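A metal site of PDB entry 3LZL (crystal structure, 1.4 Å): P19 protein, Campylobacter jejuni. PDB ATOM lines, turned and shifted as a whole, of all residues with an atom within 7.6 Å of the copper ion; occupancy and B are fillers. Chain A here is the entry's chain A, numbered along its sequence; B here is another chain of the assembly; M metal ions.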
ATOM      1  N   LEU A  22      -7.900  20.471 -19.546  1.00  0.00           N
ATOM      2  CA  LEU A  22      -9.161  21.087 -19.216  1.00  0.00           C
ATOM      3  C   LEU A  22     -10.288  20.134 -19.620  1.00  0.00           C
ATOM      4  O   LEU A  22     -10.051  18.966 -19.964  1.00  0.00           O
ATOM      5  CB  LEU A  22      -9.272  22.476 -19.818  1.00  0.00           C
ATOM      6  CG  LEU A  22      -9.041  22.704 -21.297  1.00  0.00           C
ATOM      7  CD1 LEU A  22     -10.224  22.253 -22.087  1.00  0.00           C
ATOM      8  CD2 LEU A  22      -8.867  24.172 -21.496  1.00  0.00           C
ATOM      9  N   ILE A  25     -13.364  19.470 -25.382  1.00  0.00           N
ATOM     10  CA  ILE A  25     -13.702  20.555 -26.279  1.00  0.00           C
ATOM     11  C   ILE A  25     -14.292  19.962 -27.580  1.00  0.00           C
ATOM     12  O   ILE A  25     -14.181  18.763 -27.815  1.00  0.00           O
ATOM     13  CB  ILE A  25     -12.428  21.395 -26.567  1.00  0.00           C
ATOM     14  CG1 ILE A  25     -11.772  21.838 -25.245  1.00  0.00           C
ATOM     15  CG2 ILE A  25     -12.740  22.561 -27.429  1.00  0.00           C
ATOM     16  CD1 ILE A  25     -12.714  22.533 -24.321  1.00  0.00           C
ATOM     17  N   GLU A  26     -14.950  20.803 -28.368  1.00  0.00           N
ATOM     18  CA  GLU A  26     -15.464  20.413 -29.680  1.00  0.00           C
ATOM     19  C   GLU A  26     -14.622  21.012 -30.757  1.00  0.00           C
ATOM     20  O   GLU A  26     -14.455  22.231 -30.816  1.00  0.00           O
ATOM     21  CB  GLU A  26     -16.877  20.928 -29.865  1.00  0.00           C
ATOM     22  CG  GLU A  26     -17.871  20.408 -28.863  1.00  0.00           C
ATOM     23  CD  GLU A  26     -19.237  21.072 -28.991  1.00  0.00           C
ATOM     24  OE1 GLU A  26     -19.707  21.406 -30.117  1.00  0.00           O
ATOM     25  OE2 GLU A  26     -19.852  21.262 -27.928  1.00  0.00           O
ATOM     26  N   MET A  27     -13.989  20.159 -31.568  1.00  0.00           N
ATOM     27  CA  MET A  27     -13.094  20.654 -32.606  1.00  0.00           C
ATOM     28  C   MET A  27     -13.698  20.442 -33.983  1.00  0.00           C
ATOM     29  O   MET A  27     -14.256  19.383 -34.291  1.00  0.00           O
ATOM     30  CB  MET A  27     -11.718  19.949 -32.534  1.00  0.00           C
ATOM     31  CG  MET A  27     -10.593  20.671 -33.333  1.00  0.00           C
ATOM     32  SD  MET A  27      -9.088  19.710 -33.546  1.00  0.00           S
ATOM     33  CE  MET A  27      -9.623  18.626 -34.891  1.00  0.00           C
ATOM     34  N   ASP A  33     -10.305  14.584 -34.025  1.00  0.00           N
ATOM     35  CA  ASP A  33     -10.151  14.580 -32.561  1.00  0.00           C
ATOM     36  C   ASP A  33     -11.302  13.715 -31.993  1.00  0.00           C
ATOM     37  O   ASP A  33     -12.448  13.816 -32.488  1.00  0.00           O
ATOM     38  CB  ASP A  33     -10.291  16.032 -32.034  1.00  0.00           C
ATOM     39  CG  ASP A  33      -9.916  16.172 -30.545  1.00  0.00           C
ATOM     40  OD1 ASP A  33      -8.912  15.584 -30.134  1.00  0.00           O
ATOM     41  OD2 ASP A  33     -10.619  16.908 -29.821  1.00  0.00           O
ATOM     42  N   HIS A  42      -9.402  17.548 -22.260  1.00  0.00           N
ATOM     43  CA  HIS A  42      -8.630  18.072 -23.427  1.00  0.00           C
ATOM     44  C   HIS A  42      -7.252  18.330 -22.903  1.00  0.00           C
ATOM     45  O   HIS A  42      -7.097  19.141 -22.005  1.00  0.00           O
ATOM     46  CB  HIS A  42      -9.209  19.345 -23.993  1.00  0.00           C
ATOM     47  CG  HIS A  42      -8.683  19.692 -25.351  1.00  0.00           C
ATOM     48  ND1 HIS A  42      -8.884  18.900 -26.458  1.00  0.00           N
ATOM     49  CD2 HIS A  42      -7.994  20.785 -25.782  1.00  0.00           C
ATOM     50  CE1 HIS A  42      -8.321  19.495 -27.520  1.00  0.00           C
ATOM     51  NE2 HIS A  42      -7.805  20.648 -27.141  1.00  0.00           N
ATOM     52  N   LEU A  43      -6.236  17.651 -23.471  1.00  0.00           N
ATOM     53  CA  LEU A  43      -4.855  17.793 -23.125  1.00  0.00           C
ATOM     54  C   LEU A  43      -4.256  18.788 -24.091  1.00  0.00           C
ATOM     55  O   LEU A  43      -4.392  18.622 -25.308  1.00  0.00           O
ATOM     56  CB  LEU A  43      -4.097  16.474 -23.235  1.00  0.00           C
ATOM     57  CG  LEU A  43      -2.606  16.470 -22.982  1.00  0.00           C
ATOM     58  CD1 LEU A  43      -2.286  16.956 -21.571  1.00  0.00           C
ATOM     59  CD2 LEU A  43      -2.021  15.057 -23.240  1.00  0.00           C
ATOM     60  N   GLU A  44      -3.528  19.784 -23.564  1.00  0.00           N
ATOM     61  CA  GLU A  44      -2.846  20.783 -24.389  1.00  0.00           C
ATOM     62  C   GLU A  44      -1.359  20.822 -24.051  1.00  0.00           C
ATOM     63  O   GLU A  44      -0.978  20.808 -22.884  1.00  0.00           O
ATOM     64  CB  GLU A  44      -3.477  22.179 -24.187  1.00  0.00           C
ATOM     65  CG  GLU A  44      -4.936  22.266 -24.565  1.00  0.00           C
ATOM     66  CD  GLU A  44      -5.520  23.634 -24.456  1.00  0.00           C
ATOM     67  OE1 GLU A  44      -4.821  24.567 -23.955  1.00  0.00           O
ATOM     68  OE2 GLU A  44      -6.691  23.835 -24.894  1.00  0.00           O
ATOM     69  N   MET A  86      -2.721  17.512 -31.912  1.00  0.00           N
ATOM     70  CA  MET A  86      -2.950  18.181 -33.206  1.00  0.00           C
ATOM     71  C   MET A  86      -3.001  19.698 -33.072  1.00  0.00           C
ATOM     72  O   MET A  86      -3.469  20.229 -32.081  1.00  0.00           O
ATOM     73  CB  MET A  86      -4.254  17.665 -33.829  1.00  0.00           C
ATOM     74  CG  MET A  86      -4.162  16.198 -34.189  1.00  0.00           C
ATOM     75  SD  MET A  86      -3.151  15.836 -35.637  1.00  0.00           S
ATOM     76  CE  MET A  86      -1.455  15.969 -35.084  1.00  0.00           C
ATOM     77  N   PRO A  87      -2.475  20.417 -34.069  1.00  0.00           N
ATOM     78  CA  PRO A  87      -2.488  21.876 -34.000  1.00  0.00           C
ATOM     79  C   PRO A  87      -3.886  22.450 -34.219  1.00  0.00           C
ATOM     80  O   PRO A  87      -4.616  22.006 -35.104  1.00  0.00           O
ATOM     81  CB  PRO A  87      -1.567  22.280 -35.140  1.00  0.00           C
ATOM     82  CG  PRO A  87      -1.714  21.173 -36.140  1.00  0.00           C
ATOM     83  CD  PRO A  87      -1.847  19.940 -35.302  1.00  0.00           C
ATOM     84  N   MET A  88      -4.252  23.406 -33.373  1.00  0.00           N
ATOM     85  CA  MET A  88      -5.571  24.005 -33.441  1.00  0.00           C
ATOM     86  C   MET A  88      -5.575  25.329 -32.698  1.00  0.00           C
ATOM     87  O   MET A  88      -4.582  25.684 -32.027  1.00  0.00           O
ATOM     88  CB  MET A  88      -6.586  23.061 -32.841  1.00  0.00           C
ATOM     89  CG  MET A  88      -6.419  22.844 -31.381  1.00  0.00           C
ATOM     90  SD  MET A  88      -7.495  21.582 -30.680  1.00  0.00           S
ATOM     91  CE  MET A  88      -6.620  20.123 -31.101  1.00  0.00           C
ATOM     92  N   VAL A  89      -6.665  26.069 -32.864  1.00  0.00           N
ATOM     93  CA  VAL A  89      -6.790  27.359 -32.186  1.00  0.00           C
ATOM     94  C   VAL A  89      -8.049  27.365 -31.283  1.00  0.00           C
ATOM     95  O   VAL A  89      -9.131  26.867 -31.667  1.00  0.00           O
ATOM     96  CB  VAL A  89      -6.755  28.552 -33.180  1.00  0.00           C
ATOM     97  CG1 VAL A  89      -8.012  28.613 -34.100  1.00  0.00           C
ATOM     98  CG2 VAL A  89      -6.580  29.892 -32.432  1.00  0.00           C
ATOM     99  N   ALA A  90      -7.893  27.978 -30.125  1.00  0.00           N
ATOM    100  CA  ALA A  90      -8.999  28.216 -29.191  1.00  0.00           C
ATOM    101  C   ALA A  90      -9.042  29.724 -28.860  1.00  0.00           C
ATOM    102  O   ALA A  90      -8.282  30.533 -29.458  1.00  0.00           O
ATOM    103  CB  ALA A  90      -8.866  27.357 -27.927  1.00  0.00           C
ATOM    104  N   ASP A  92      -8.003  31.294 -26.515  1.00  0.00           N
ATOM    105  CA  ASP A  92      -6.689  31.662 -25.945  1.00  0.00           C
ATOM    106  C   ASP A  92      -5.496  31.419 -26.866  1.00  0.00           C
ATOM    107  O   ASP A  92      -4.372  31.451 -26.430  1.00  0.00           O
ATOM    108  CB  ASP A  92      -6.490  31.083 -24.528  1.00  0.00           C
ATOM    109  CG  ASP A  92      -6.484  29.588 -24.459  1.00  0.00           C
ATOM    110  OD1 ASP A  92      -6.755  28.900 -25.440  1.00  0.00           O
ATOM    111  OD2 ASP A  92      -6.206  29.062 -23.346  1.00  0.00           O
ATOM    112  N   GLY A  93      -5.769  31.209 -28.161  1.00  0.00           N
ATOM    113  CA  GLY A  93      -4.784  31.117 -29.205  1.00  0.00           C
ATOM    114  C   GLY A  93      -4.434  29.705 -29.635  1.00  0.00           C
ATOM    115  O   GLY A  93      -5.053  28.722 -29.195  1.00  0.00           O
ATOM    116  N   PRO A  94      -3.383  29.565 -30.477  1.00  0.00           N
ATOM    117  CA  PRO A  94      -3.028  28.252 -31.022  1.00  0.00           C
ATOM    118  C   PRO A  94      -2.316  27.417 -29.993  1.00  0.00           C
ATOM    119  O   PRO A  94      -1.637  27.968 -29.084  1.00  0.00           O
ATOM    120  CB  PRO A  94      -2.088  28.602 -32.171  1.00  0.00           C
ATOM    121  CG  PRO A  94      -1.469  29.916 -31.763  1.00  0.00           C
ATOM    122  CD  PRO A  94      -2.597  30.650 -31.104  1.00  0.00           C
ATOM    123  N   HIS A  95      -2.503  26.092 -30.080  1.00  0.00           N
ATOM    124  CA  HIS A  95      -1.823  25.116 -29.246  1.00  0.00           C
ATOM    125  C   HIS A  95      -1.883  23.767 -29.958  1.00  0.00           C
ATOM    126  O   HIS A  95      -2.388  23.669 -31.086  1.00  0.00           O
ATOM    127  CB  HIS A  95      -2.512  24.991 -27.851  1.00  0.00           C
ATOM    128  CG  HIS A  95      -3.952  24.533 -27.958  1.00  0.00           C
ATOM    129  ND1 HIS A  95      -5.017  25.391 -27.895  1.00  0.00           N
ATOM    130  CD2 HIS A  95      -4.478  23.296 -28.066  1.00  0.00           C
ATOM    131  CE1 HIS A  95      -6.138  24.699 -27.985  1.00  0.00           C
ATOM    132  NE2 HIS A  95      -5.831  23.432 -28.166  1.00  0.00           N
ATOM    133  N   TYR A  96      -1.283  22.750 -29.323  1.00  0.00           N
ATOM    134  CA  TYR A  96      -1.395  21.365 -29.769  1.00  0.00           C
ATOM    135  C   TYR A  96      -2.241  20.660 -28.742  1.00  0.00           C
ATOM    136  O   TYR A  96      -1.990  20.801 -27.535  1.00  0.00           O
ATOM    137  CB  TYR A  96       0.010  20.730 -29.856  1.00  0.00           C
ATOM    138  CG  TYR A  96       0.926  21.385 -30.854  1.00  0.00           C
ATOM    139  CD1 TYR A  96       0.957  21.009 -32.162  1.00  0.00           C
ATOM    140  CD2 TYR A  96       1.781  22.381 -30.466  1.00  0.00           C
ATOM    141  CE1 TYR A  96       1.764  21.630 -33.094  1.00  0.00           C
ATOM    142  CE2 TYR A  96       2.597  23.028 -31.367  1.00  0.00           C
ATOM    143  CZ  TYR A  96       2.612  22.615 -32.704  1.00  0.00           C
ATOM    144  OH  TYR A  96       3.395  23.233 -33.637  1.00  0.00           O
ATOM    145  N   GLY A  97      -3.257  19.926 -29.180  1.00  0.00           N
ATOM    146  CA  GLY A  97      -4.165  19.319 -28.213  1.00  0.00           C
ATOM    147  C   GLY A  97      -4.833  18.042 -28.697  1.00  0.00           C
ATOM    148  O   GLY A  97      -4.733  17.671 -29.857  1.00  0.00           O
ATOM    149  N   ALA A  98      -5.474  17.371 -27.753  1.00  0.00           N
ATOM    150  CA  ALA A  98      -6.274  16.166 -28.035  1.00  0.00           C
ATOM    151  C   ALA A  98      -7.279  15.958 -26.934  1.00  0.00           C
ATOM    152  O   ALA A  98      -6.939  16.047 -25.740  1.00  0.00           O
ATOM    153  CB  ALA A  98      -5.371  14.935 -28.113  1.00  0.00           C
ATOM    154  N   ASN A  99      -8.507  15.616 -27.323  1.00  0.00           N
ATOM    155  CA  ASN A  99      -9.485  15.043 -26.382  1.00  0.00           C
ATOM    156  C   ASN A  99      -9.052  13.625 -26.017  1.00  0.00           C
ATOM    157  O   ASN A  99      -8.629  12.854 -26.893  1.00  0.00           O
ATOM    158  CB  ASN A  99     -10.931  15.054 -26.945  1.00  0.00           C
ATOM    159  CG  ASN A  99     -11.633  16.339 -26.803  1.00  0.00           C
ATOM    160  OD1 ASN A  99     -11.213  17.307 -26.164  1.00  0.00           O
ATOM    161  ND2 ASN A  99     -12.813  16.341 -27.409  1.00  0.00           N
ATOM    162  N   GLY B 130      -7.075  22.805 -36.752  1.00  0.00           N
ATOM    163  CA  GLY B 130      -8.341  22.718 -36.105  1.00  0.00           C
ATOM    164  C   GLY B 130      -8.748  23.986 -35.386  1.00  0.00           C
ATOM    165  O   GLY B 130      -7.939  24.923 -35.190  1.00  0.00           O
ATOM    166  N   ARG B 131     -10.020  24.052 -35.039  1.00  0.00           N
ATOM    167  CA  ARG B 131     -10.548  25.131 -34.199  1.00  0.00           C
ATOM    168  C   ARG B 131     -11.547  24.620 -33.207  1.00  0.00           C
ATOM    169  O   ARG B 131     -12.389  23.750 -33.541  1.00  0.00           O
ATOM    170  CB  ARG B 131     -11.091  26.301 -35.030  1.00  0.00           C
ATOM    171  CG  ARG B 131     -12.385  26.095 -35.684  1.00  0.00           C
ATOM    172  CD  ARG B 131     -12.881  27.324 -36.410  1.00  0.00           C
ATOM    173  NE  ARG B 131     -14.163  26.919 -36.947  1.00  0.00           N
ATOM    174  CZ  ARG B 131     -15.349  27.333 -36.548  1.00  0.00           C
ATOM    175  NH1 ARG B 131     -15.512  28.250 -35.603  1.00  0.00           N
ATOM    176  NH2 ARG B 131     -16.403  26.858 -37.168  1.00  0.00           N
ATOM    177  N   HIS B 132     -11.456  25.136 -31.973  1.00  0.00           N
ATOM    178  CA  HIS B 132     -12.482  24.894 -30.990  1.00  0.00           C
ATOM    179  C   HIS B 132     -13.756  25.615 -31.415  1.00  0.00           C
ATOM    180  O   HIS B 132     -13.700  26.760 -31.804  1.00  0.00           O
ATOM    181  CB  HIS B 132     -12.068  25.345 -29.566  1.00  0.00           C
ATOM    182  CG  HIS B 132     -10.872  24.656 -28.985  1.00  0.00           C
ATOM    183  ND1 HIS B 132     -10.711  24.546 -27.627  1.00  0.00           N
ATOM    184  CD2 HIS B 132      -9.924  23.894 -29.546  1.00  0.00           C
ATOM    185  CE1 HIS B 132      -9.578  23.847 -27.381  1.00  0.00           C
ATOM    186  NE2 HIS B 132      -9.092  23.446 -28.551  1.00  0.00           N
ATOM    187  N   THR B 137     -14.750  27.675 -25.081  1.00  0.00           N
ATOM    188  CA  THR B 137     -13.394  27.976 -25.589  1.00  0.00           C
ATOM    189  C   THR B 137     -13.322  28.224 -27.080  1.00  0.00           C
ATOM    190  O   THR B 137     -12.222  28.442 -27.620  1.00  0.00           O
ATOM    191  CB  THR B 137     -12.449  26.823 -25.255  1.00  0.00           C
ATOM    192  OG1 THR B 137     -12.681  25.705 -26.127  1.00  0.00           O
ATOM    193  CG2 THR B 137     -12.694  26.368 -23.800  1.00  0.00           C
HETATM  194 CU    CU M   1      -7.429  22.120 -28.474  1.00  0.00          CU
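OG1 of Thr 137 of chain B is in hydrogen-bond range of ND1 of His 132 of chain B, at 2.7 Å. The backbone carbonyl oxygen of Leu 22 sits at hydrogen-bond distance from the backbone NH of His 42, 2.8 Å away. A ring nitrogen (ND1) of His 42 is in hydrogen-bond range of the side-chain amide oxygen (OD1) of Asn 99, 2.8 Å away. The backbone carbonyl oxygen of Val 89 sits at hydrogen-bond distance from the backbone NH of His 132 of chain B (2.9 Å). OE2 of Glu 44 sits close to NE2 of His 95 (3.4 Å).
The nearest printed residue that does not touch the copper ion is Glu 44 (4.04 Å).
NE2 of His 42 binds the copper ion, at 2.0 Å. The copper ion is bound by NE2 of His 95, at 2.1 Å. The copper ion is bound by a ring nitrogen (NE2) of His 132 of chain B (2.1 Å). SD of Met 88 binds the copper ion, 2.3 Å away. The copper ion has four donor atoms within binding distance.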
